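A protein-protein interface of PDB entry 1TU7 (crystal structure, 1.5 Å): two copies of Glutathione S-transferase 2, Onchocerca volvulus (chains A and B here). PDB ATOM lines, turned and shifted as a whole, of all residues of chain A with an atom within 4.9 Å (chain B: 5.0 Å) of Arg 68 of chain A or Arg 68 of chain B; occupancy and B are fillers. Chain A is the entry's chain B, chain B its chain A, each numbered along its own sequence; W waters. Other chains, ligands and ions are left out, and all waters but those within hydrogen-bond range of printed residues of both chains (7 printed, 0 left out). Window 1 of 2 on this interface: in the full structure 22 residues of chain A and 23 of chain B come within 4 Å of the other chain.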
ATOM      1  N   GLY A  64     -14.777 -11.157  -2.521  1.00  0.00           N
ATOM      2  CA  GLY A  64     -13.652 -11.930  -2.990  1.00  0.00           C
ATOM      3  C   GLY A  64     -13.314 -11.639  -4.432  1.00  0.00           C
ATOM      4  O   GLY A  64     -12.138 -11.570  -4.838  1.00  0.00           O
ATOM      5  N   ALA A  65     -14.346 -11.480  -5.246  1.00  0.00           N
ATOM      6  CA  ALA A  65     -14.171 -11.166  -6.651  1.00  0.00           C
ATOM      7  C   ALA A  65     -13.617  -9.747  -6.827  1.00  0.00           C
ATOM      8  O   ALA A  65     -12.766  -9.498  -7.687  1.00  0.00           O
ATOM      9  CB  ALA A  65     -15.475 -11.334  -7.420  1.00  0.00           C
ATOM     10  N   ILE A  66     -14.082  -8.810  -6.007  1.00  0.00           N
ATOM     11  CA  ILE A  66     -13.601  -7.450  -6.083  1.00  0.00           C
ATOM     12  C   ILE A  66     -12.112  -7.444  -5.788  1.00  0.00           C
ATOM     13  O   ILE A  66     -11.303  -6.850  -6.524  1.00  0.00           O
ATOM     14  CB  ILE A  66     -14.333  -6.547  -5.079  1.00  0.00           C
ATOM     15  CG1 ILE A  66     -15.779  -6.326  -5.474  1.00  0.00           C
ATOM     16  CG2 ILE A  66     -13.606  -5.199  -4.932  1.00  0.00           C
ATOM     17  CD1 ILE A  66     -16.626  -5.828  -4.357  1.00  0.00           C
ATOM     18  N   LEU A  67     -11.703  -8.102  -4.706  1.00  0.00           N
ATOM     19  CA  LEU A  67     -10.288  -8.056  -4.313  1.00  0.00           C
ATOM     20  C   LEU A  67      -9.410  -8.768  -5.330  1.00  0.00           C
ATOM     21  O   LEU A  67      -8.329  -8.294  -5.654  1.00  0.00           O
ATOM     22  CB  LEU A  67     -10.123  -8.615  -2.889  1.00  0.00           C
ATOM     23  CG  LEU A  67      -8.762  -8.457  -2.235  1.00  0.00           C
ATOM     24  CD1 LEU A  67      -8.345  -7.002  -2.096  1.00  0.00           C
ATOM     25  CD2 LEU A  67      -8.740  -9.193  -0.878  1.00  0.00           C
ATOM     26  N   ARG A  68      -9.873  -9.893  -5.862  1.00  0.00           N
ATOM     27  CA  ARG A  68      -9.089 -10.596  -6.850  1.00  0.00           C
ATOM     28  C   ARG A  68      -8.953  -9.802  -8.144  1.00  0.00           C
ATOM     29  O   ARG A  68      -7.904  -9.858  -8.813  1.00  0.00           O
ATOM     30  CB  ARG A  68      -9.674 -11.983  -7.121  1.00  0.00           C
ATOM     31  CG  ARG A  68      -9.291 -13.013  -6.051  1.00  0.00           C
ATOM     32  CD  ARG A  68      -9.791 -14.401  -6.359  1.00  0.00           C
ATOM     33  NE  ARG A  68     -11.244 -14.557  -6.265  1.00  0.00           N
ATOM     34  CZ  ARG A  68     -11.915 -14.848  -5.159  1.00  0.00           C
ATOM     35  NH1 ARG A  68     -11.291 -14.999  -3.979  1.00  0.00           N
ATOM     36  NH2 ARG A  68     -13.237 -14.930  -5.226  1.00  0.00           N
ATOM     37  N   HIS A  69      -9.988  -9.066  -8.507  1.00  0.00           N
ATOM     38  CA  HIS A  69      -9.941  -8.174  -9.659  1.00  0.00           C
ATOM     39  C   HIS A  69      -8.928  -7.058  -9.456  1.00  0.00           C
ATOM     40  O   HIS A  69      -8.112  -6.787 -10.330  1.00  0.00           O
ATOM     41  CB  HIS A  69     -11.341  -7.601  -9.903  1.00  0.00           C
ATOM     42  CG  HIS A  69     -11.357  -6.435 -10.820  1.00  0.00           C
ATOM     43  ND1 HIS A  69     -11.622  -5.133 -10.434  1.00  0.00           N
ATOM     44  CD2 HIS A  69     -11.075  -6.388 -12.140  1.00  0.00           C
ATOM     45  CE1 HIS A  69     -11.539  -4.347 -11.504  1.00  0.00           C
ATOM     46  NE2 HIS A  69     -11.221  -5.087 -12.547  1.00  0.00           N
ATOM     47  N   LEU A  70      -8.985  -6.393  -8.309  1.00  0.00           N
ATOM     48  CA  LEU A  70      -8.028  -5.349  -8.003  1.00  0.00           C
ATOM     49  C   LEU A  70      -6.605  -5.895  -8.036  1.00  0.00           C
ATOM     50  O   LEU A  70      -5.711  -5.251  -8.548  1.00  0.00           O
ATOM     51  CB  LEU A  70      -8.328  -4.723  -6.632  1.00  0.00           C
ATOM     52  CG  LEU A  70      -9.537  -3.787  -6.695  1.00  0.00           C
ATOM     53  CD1 LEU A  70      -9.898  -3.401  -5.284  1.00  0.00           C
ATOM     54  CD2 LEU A  70      -9.308  -2.525  -7.571  1.00  0.00           C
ATOM     55  N   ALA A  71      -6.415  -7.092  -7.521  1.00  0.00           N
ATOM     56  CA  ALA A  71      -5.100  -7.711  -7.461  1.00  0.00           C
ATOM     57  C   ALA A  71      -4.550  -7.902  -8.860  1.00  0.00           C
ATOM     58  O   ALA A  71      -3.382  -7.638  -9.097  1.00  0.00           O
ATOM     59  CB  ALA A  71      -5.173  -9.050  -6.752  1.00  0.00           C
ATOM     60  N   ARG A  72      -5.371  -8.359  -9.790  1.00  0.00           N
ATOM     61  CA  ARG A  72      -4.897  -8.527 -11.169  1.00  0.00           C
ATOM     62  C   ARG A  72      -4.552  -7.186 -11.797  1.00  0.00           C
ATOM     63  O   ARG A  72      -3.487  -6.990 -12.392  1.00  0.00           O
ATOM     64  CB  ARG A  72      -5.934  -9.259 -12.017  1.00  0.00           C
ATOM     65  CG  ARG A  72      -6.060 -10.712 -11.723  1.00  0.00           C
ATOM     66  CD  ARG A  72      -6.975 -11.417 -12.697  1.00  0.00           C
ATOM     67  NE  ARG A  72      -8.346 -10.913 -12.637  1.00  0.00           N
ATOM     68  CZ  ARG A  72      -9.279 -11.417 -11.825  1.00  0.00           C
ATOM     69  NH1 ARG A  72     -10.491 -10.913 -11.858  1.00  0.00           N
ATOM     70  NH2 ARG A  72      -9.012 -12.405 -10.981  1.00  0.00           N
ATOM     71  N   ASP A  88      -4.321 -17.241  -3.223  1.00  0.00           N
ATOM     72  CA  ASP A  88      -5.768 -17.493  -3.315  1.00  0.00           C
ATOM     73  C   ASP A  88      -6.176 -18.456  -2.195  1.00  0.00           C
ATOM     74  O   ASP A  88      -7.079 -18.214  -1.376  1.00  0.00           O
ATOM     75  CB  ASP A  88      -6.061 -18.044  -4.709  1.00  0.00           C
ATOM     76  CG  ASP A  88      -7.512 -18.100  -5.049  1.00  0.00           C
ATOM     77  OD1 ASP A  88      -8.391 -17.847  -4.192  1.00  0.00           O
ATOM     78  OD2 ASP A  88      -7.821 -18.456  -6.218  1.00  0.00           O
ATOM     79  N   GLU A  92      -8.492 -17.366   0.891  1.00  0.00           N
ATOM     80  CA  GLU A  92      -9.707 -18.135   1.169  1.00  0.00           C
ATOM     81  C   GLU A  92      -9.705 -18.708   2.569  1.00  0.00           C
ATOM     82  O   GLU A  92     -10.747 -18.802   3.203  1.00  0.00           O
ATOM     83  CB  GLU A  92      -9.879 -19.260   0.154  1.00  0.00           C
ATOM     84  CG  GLU A  92     -10.221 -18.764  -1.232  1.00  0.00           C
ATOM     85  CD  GLU A  92     -11.624 -18.217  -1.317  1.00  0.00           C
ATOM     86  OE1 GLU A  92     -12.557 -19.040  -1.260  1.00  0.00           O
ATOM     87  OE2 GLU A  92     -11.796 -16.994  -1.416  1.00  0.00           O
ATOM     88  N   TYR A 149      -2.523  -9.161  -2.515  1.00  0.00           N
ATOM     89  CA  TYR A 149      -3.802  -8.828  -1.957  1.00  0.00           C
ATOM     90  C   TYR A 149      -4.085  -9.576  -0.659  1.00  0.00           C
ATOM     91  O   TYR A 149      -4.820  -9.070   0.200  1.00  0.00           O
ATOM     92  CB  TYR A 149      -4.918  -9.065  -2.946  1.00  0.00           C
ATOM     93  CG  TYR A 149      -5.217 -10.492  -3.302  1.00  0.00           C
ATOM     94  CD1 TYR A 149      -6.220 -11.183  -2.649  1.00  0.00           C
ATOM     95  CD2 TYR A 149      -4.564 -11.143  -4.339  1.00  0.00           C
ATOM     96  CE1 TYR A 149      -6.560 -12.511  -3.000  1.00  0.00           C
ATOM     97  CE2 TYR A 149      -4.909 -12.440  -4.694  1.00  0.00           C
ATOM     98  CZ  TYR A 149      -5.888 -13.119  -4.029  1.00  0.00           C
ATOM     99  OH  TYR A 149      -6.203 -14.410  -4.418  1.00  0.00           O
ATOM    100  N   GLY B  64     -12.335 -22.945  -3.948  1.00  0.00           N
ATOM    101  CA  GLY B  64     -12.291 -21.877  -4.924  1.00  0.00           C
ATOM    102  C   GLY B  64     -10.935 -21.670  -5.551  1.00  0.00           C
ATOM    103  O   GLY B  64     -10.800 -21.361  -6.733  1.00  0.00           O
ATOM    104  N   ALA B  65      -9.886 -21.846  -4.753  1.00  0.00           N
ATOM    105  CA  ALA B  65      -8.519 -21.732  -5.267  1.00  0.00           C
ATOM    106  C   ALA B  65      -8.192 -22.884  -6.214  1.00  0.00           C
ATOM    107  O   ALA B  65      -7.528 -22.697  -7.211  1.00  0.00           O
ATOM    108  CB  ALA B  65      -7.499 -21.694  -4.133  1.00  0.00           C
ATOM    109  N   ILE B  66      -8.704 -24.070  -5.898  1.00  0.00           N
ATOM    110  CA  ILE B  66      -8.524 -25.236  -6.756  1.00  0.00           C
ATOM    111  C   ILE B  66      -9.178 -24.972  -8.099  1.00  0.00           C
ATOM    112  O   ILE B  66      -8.570 -25.165  -9.157  1.00  0.00           O
ATOM    113  CB  ILE B  66      -9.114 -26.512  -6.093  1.00  0.00           C
ATOM    114  CG1 ILE B  66      -8.334 -26.914  -4.837  1.00  0.00           C
ATOM    115  CG2 ILE B  66      -9.154 -27.655  -7.115  1.00  0.00           C
ATOM    116  CD1 ILE B  66      -9.045 -27.921  -3.944  1.00  0.00           C
ATOM    117  N   LEU B  67     -10.424 -24.530  -8.059  1.00  0.00           N
ATOM    118  CA  LEU B  67     -11.155 -24.266  -9.289  1.00  0.00           C
ATOM    119  C   LEU B  67     -10.476 -23.200 -10.154  1.00  0.00           C
ATOM    120  O   LEU B  67     -10.373 -23.360 -11.368  1.00  0.00           O
ATOM    121  CB  LEU B  67     -12.581 -23.865  -8.951  1.00  0.00           C
ATOM    122  CG  LEU B  67     -13.845 -24.346  -9.600  1.00  0.00           C
ATOM    123  CD1 LEU B  67     -13.767 -25.752 -10.158  1.00  0.00           C
ATOM    124  CD2 LEU B  67     -14.908 -24.202  -8.499  1.00  0.00           C
ATOM    125  N   ARG B  68     -10.035 -22.102  -9.545  1.00  0.00           N
ATOM    126  CA  ARG B  68      -9.378 -21.050 -10.333  1.00  0.00           C
ATOM    127  C   ARG B  68      -8.031 -21.491 -10.878  1.00  0.00           C
ATOM    128  O   ARG B  68      -7.636 -21.107 -11.962  1.00  0.00           O
ATOM    129  CB  ARG B  68      -9.230 -19.758  -9.528  1.00  0.00           C
ATOM    130  CG  ARG B  68     -10.542 -19.015  -9.430  1.00  0.00           C
ATOM    131  CD  ARG B  68     -10.458 -17.723  -8.672  1.00  0.00           C
ATOM    132  NE  ARG B  68     -10.368 -17.960  -7.264  1.00  0.00           N
ATOM    133  CZ  ARG B  68     -11.403 -18.138  -6.462  1.00  0.00           C
ATOM    134  NH1 ARG B  68     -12.645 -18.113  -7.005  1.00  0.00           N
ATOM    135  NH2 ARG B  68     -11.236 -18.363  -5.181  1.00  0.00           N
ATOM    136  N   HIS B  69      -7.300 -22.321 -10.137  1.00  0.00           N
ATOM    137  CA  HIS B  69      -6.058 -22.851 -10.652  1.00  0.00           C
ATOM    138  C   HIS B  69      -6.297 -23.725 -11.875  1.00  0.00           C
ATOM    139  O   HIS B  69      -5.636 -23.597 -12.886  1.00  0.00           O
ATOM    140  CB  HIS B  69      -5.327 -23.634  -9.569  1.00  0.00           C
ATOM    141  CG  HIS B  69      -4.269 -24.535 -10.076  1.00  0.00           C
ATOM    142  ND1 HIS B  69      -3.017 -24.087 -10.414  1.00  0.00           N
ATOM    143  CD2 HIS B  69      -4.266 -25.877 -10.298  1.00  0.00           C
ATOM    144  CE1 HIS B  69      -2.281 -25.107 -10.817  1.00  0.00           C
ATOM    145  NE2 HIS B  69      -3.009 -26.207 -10.743  1.00  0.00           N
ATOM    146  N   LEU B  70      -7.259 -24.637 -11.774  1.00  0.00           N
ATOM    147  CA  LEU B  70      -7.584 -25.467 -12.909  1.00  0.00           C
ATOM    148  C   LEU B  70      -8.065 -24.623 -14.096  1.00  0.00           C
ATOM    149  O   LEU B  70      -7.698 -24.893 -15.253  1.00  0.00           O
ATOM    150  CB  LEU B  70      -8.631 -26.488 -12.514  1.00  0.00           C
ATOM    151  CG  LEU B  70      -8.130 -27.627 -11.625  1.00  0.00           C
ATOM    152  CD1 LEU B  70      -9.340 -28.423 -11.174  1.00  0.00           C
ATOM    153  CD2 LEU B  70      -7.144 -28.490 -12.363  1.00  0.00           C
ATOM    154  N   ALA B  71      -8.879 -23.612 -13.795  1.00  0.00           N
ATOM    155  CA  ALA B  71      -9.386 -22.720 -14.822  1.00  0.00           C
ATOM    156  C   ALA B  71      -8.257 -22.024 -15.572  1.00  0.00           C
ATOM    157  O   ALA B  71      -8.296 -21.930 -16.796  1.00  0.00           O
ATOM    158  CB  ALA B  71     -10.292 -21.730 -14.219  1.00  0.00           C
ATOM    159  N   ARG B  72      -7.256 -21.507 -14.881  1.00  0.00           N
ATOM    160  CA  ARG B  72      -6.123 -20.865 -15.574  1.00  0.00           C
ATOM    161  C   ARG B  72      -5.358 -21.885 -16.430  1.00  0.00           C
ATOM    162  O   ARG B  72      -5.037 -21.614 -17.578  1.00  0.00           O
ATOM    163  CB  ARG B  72      -5.184 -20.190 -14.582  1.00  0.00           C
ATOM    164  CG  ARG B  72      -5.729 -18.909 -14.012  1.00  0.00           C
ATOM    165  CD  ARG B  72      -4.735 -18.174 -13.109  1.00  0.00           C
ATOM    166  NE  ARG B  72      -4.367 -18.959 -11.924  1.00  0.00           N
ATOM    167  CZ  ARG B  72      -4.979 -18.888 -10.764  1.00  0.00           C
ATOM    168  NH1 ARG B  72      -6.002 -18.067 -10.593  1.00  0.00           N
ATOM    169  NH2 ARG B  72      -4.581 -19.644  -9.732  1.00  0.00           N
ATOM    170  N   ASN B  77     -10.996 -19.617 -17.535  1.00  0.00           N
ATOM    171  CA  ASN B  77     -11.005 -18.446 -16.638  1.00  0.00           C
ATOM    172  C   ASN B  77     -11.375 -17.163 -17.381  1.00  0.00           C
ATOM    173  O   ASN B  77     -11.003 -16.093 -16.943  1.00  0.00           O
ATOM    174  CB  ASN B  77      -9.609 -18.294 -16.040  1.00  0.00           C
ATOM    175  CG  ASN B  77      -9.554 -17.399 -14.822  1.00  0.00           C
ATOM    176  OD1 ASN B  77      -8.518 -16.742 -14.595  1.00  0.00           O
ATOM    177  ND2 ASN B  77     -10.550 -17.455 -13.995  1.00  0.00           N
ATOM    178  N   ASP B  88     -15.995 -15.064 -11.687  1.00  0.00           N
ATOM    179  CA  ASP B  88     -15.663 -15.146 -10.263  1.00  0.00           C
ATOM    180  C   ASP B  88     -16.817 -14.632  -9.452  1.00  0.00           C
ATOM    181  O   ASP B  88     -17.308 -15.284  -8.535  1.00  0.00           O
ATOM    182  CB  ASP B  88     -14.396 -14.330 -10.052  1.00  0.00           C
ATOM    183  CG  ASP B  88     -13.817 -14.415  -8.706  1.00  0.00           C
ATOM    184  OD1 ASP B  88     -14.376 -15.086  -7.804  1.00  0.00           O
ATOM    185  OD2 ASP B  88     -12.733 -13.784  -8.501  1.00  0.00           O
ATOM    186  N   GLU B  92     -19.009 -16.831  -6.923  1.00  0.00           N
ATOM    187  CA  GLU B  92     -19.166 -16.427  -5.532  1.00  0.00           C
ATOM    188  C   GLU B  92     -20.634 -16.337  -5.133  1.00  0.00           C
ATOM    189  O   GLU B  92     -20.999 -16.692  -4.005  1.00  0.00           O
ATOM    190  CB  GLU B  92     -18.445 -15.117  -5.238  1.00  0.00           C
ATOM    191  CG  GLU B  92     -16.924 -15.233  -5.256  1.00  0.00           C
ATOM    192  CD  GLU B  92     -16.401 -16.117  -4.148  1.00  0.00           C
ATOM    193  OE1 GLU B  92     -15.925 -17.213  -4.462  1.00  0.00           O
ATOM    194  OE2 GLU B  92     -16.589 -15.715  -2.968  1.00  0.00           O
ATOM    195  N   TYR B 149     -15.184 -22.116 -15.427  1.00  0.00           N
ATOM    196  CA  TYR B 149     -15.318 -22.906 -14.225  1.00  0.00           C
ATOM    197  C   TYR B 149     -16.648 -22.653 -13.528  1.00  0.00           C
ATOM    198  O   TYR B 149     -17.176 -23.552 -12.867  1.00  0.00           O
ATOM    199  CB  TYR B 149     -14.169 -22.705 -13.260  1.00  0.00           C
ATOM    200  CG  TYR B 149     -14.032 -21.342 -12.628  1.00  0.00           C
ATOM    201  CD1 TYR B 149     -14.606 -21.075 -11.387  1.00  0.00           C
ATOM    202  CD2 TYR B 149     -13.289 -20.327 -13.228  1.00  0.00           C
ATOM    203  CE1 TYR B 149     -14.482 -19.861 -10.781  1.00  0.00           C
ATOM    204  CE2 TYR B 149     -13.126 -19.098 -12.589  1.00  0.00           C
ATOM    205  CZ  TYR B 149     -13.725 -18.868 -11.368  1.00  0.00           C
ATOM    206  OH  TYR B 149     -13.537 -17.644 -10.746  1.00  0.00           O
HETATM  207  O   HOH W   1     -13.870 -18.784  -3.778  1.00  0.00           O
HETATM  208  O   HOH W   2     -13.862 -15.434  -2.312  1.00  0.00           O
HETATM  209  O   HOH W   3     -12.396 -11.357  -9.736  1.00  0.00           O
HETATM  210  O   HOH W   4     -16.908 -13.009  -2.599  1.00  0.00           O
HETATM  211  O   HOH W   5      -6.118 -20.308  -7.431  1.00  0.00           O
HETATM  212  O   HOH W   6      -6.724 -16.791  -8.085  1.00  0.00           O
HETATM  213  O   HOH W   7     -12.259 -21.707  -1.366  1.00  0.00           O
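Printed residues of chain B that touch a printed residue of chain A: Ala 65, Arg 68, Asp 88 and Glu 92. Hydrophobic or aromatic side chains of chain B that line the printed part of chain A: Ala 65. Along chain B the printed residues that touch a printed residue of chain A span positions 65 to 92. Among the printed residues, Asp or Glu carboxylates within 4 Å of a Lys or Arg side-chain nitrogen of the other chain: Arg 68 of chain A with Asp 88 of chain B (2.8 Å), Arg 68 of chain A with Glu 92 of chain B (3.6 Å) and Asp 88 of chain A with Arg 68 of chain B (2.8 Å).
O of Gly 64 of chain B lies close to NH2 of Arg 68 of chain B. The side-chain carboxylate (OD1) of Asp 88 of chain B is in salt-bridge range of the guanidinium group (NH1) of Arg 68 of chain B. The backbone carbonyl oxygen of Gly 64 of chain A sits close to the guanidinium group of Arg 68 of chain A (3.4 Å). The guanidinium group of Arg 68 of chain A is in salt-bridge range of the side-chain carboxylate of Glu 92 of chain A (3.3 Å).
OD2 of Asp 88 of chain A is in salt-bridge range of NE of Arg 68 of chain B, 2.8 Å away. The side-chain carboxylate of Asp 88 of chain B lies within salt-bridge range of the guanidinium group of Arg 68 of chain A (2.8 Å). The side-chain carboxylate of Glu 92 of chain B lies within salt-bridge range of the guanidinium group of Arg 68 of chain A (3.6 Å).
Ala 65 of chain A touches Asp 88 of chain B, and with the chains exchanged Asp 88 of chain A touches Ala 65 of chain B. Arg 68 of chain B touches its own counterpart, Arg 68 of chain A. Arg 68 of chain A touches Asp 88 of chain B, and with the chains exchanged Asp 88 of chain A touches Arg 68 of chain B. Arg 68 of chain A touches Glu 92 of chain B, and with the chains exchanged Glu 92 of chain A touches Arg 68 of chain B. Positions printed for both chains: 64, 65, 66, 67, 68, 69, 70, 71, 72, 88, 92 and 149. Of the 7 pairs that touch across the chains among the printed residues, 7 have their exchanged pair printed and touching as well.
Of chain B, only Arg 68, Asp 88 and Glu 92 come within 4 Å of Arg 68 of chain A. Printed residues of chain B within 4 Å of Asp 88 of chain A: Ala 65 and Arg 68. Printed residues of chain B within 4 Å of Glu 92 of chain A: Arg 68 (3.9 Å). Printed residues of chain A within 4 Å of Ala 65 of chain B: Asp 88 (3.5 Å). Of the printed residues of chain A, Arg 68 of chain B touches Arg 68 (3.6 Å), Asp 88 (2.8 Å) and Glu 92 (3.9 Å). Of the printed residues of chain A, Glu 92 of chain B touches Arg 68 (3.5 Å). The nearest printed residue of chain B that does not touch Arg 68 of chain A is Tyr 149 of chain B (5.9 Å). The nearest printed residue of chain A that does not touch Arg 68 of chain B is Arg 72 of chain A (6.0 Å). The nearest printed residue of chain A that does not touch Asp 88 of chain B is Gly 64 of chain A (4.3 Å).
Among the printed residues, merely in contact across the chains: Ala 65 of chain A with Asp 88 of chain B (3.5 Å), Arg 68 of chain A with Arg 68 of chain B (3.6 Å), Asp 88 of chain A with Ala 65 of chain B (3.5 Å) and Glu 92 of chain A with Arg 68 of chain B (3.9 Å).
Water W1 lies within hydrogen-bond range of OE1 of Glu 92 of chain B (2.7 Å), OE1 of Glu 92 of chain A (2.9 Å) and NH2 of Arg 68 of chain B (3.0 Å). Water W7 bridges OE1 of Glu 92 of chain A (2.7 Å) and N of Gly 64 of chain B (2.9 Å). Water W6 bridges the side-chain carboxylate (OD2) of Asp 88 of chain A (2.7 Å) and the guanidinium group (NH1) of Arg 72 of chain B (2.9 Å). Water W2 lies within hydrogen-bond range of the side-chain carboxylate (OE2) of Glu 92 of chain A (2.7 Å), the side-chain carboxylate (OE2) of Glu 92 of chain B (2.8 Å) and the guanidinium group (NH2) of Arg 68 of chain A (3.0 Å). Water W4 lies within hydrogen-bond range of OE2 of Glu 92 of chain B (2.7 Å) and N of Gly 64 of chain A (2.8 Å). Water W5 lies within hydrogen-bond range of O of Ala 65 of chain B (2.8 Å), OD2 of Asp 88 of chain A (2.8 Å) and NH2 of Arg 72 of chain B (2.8 Å).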
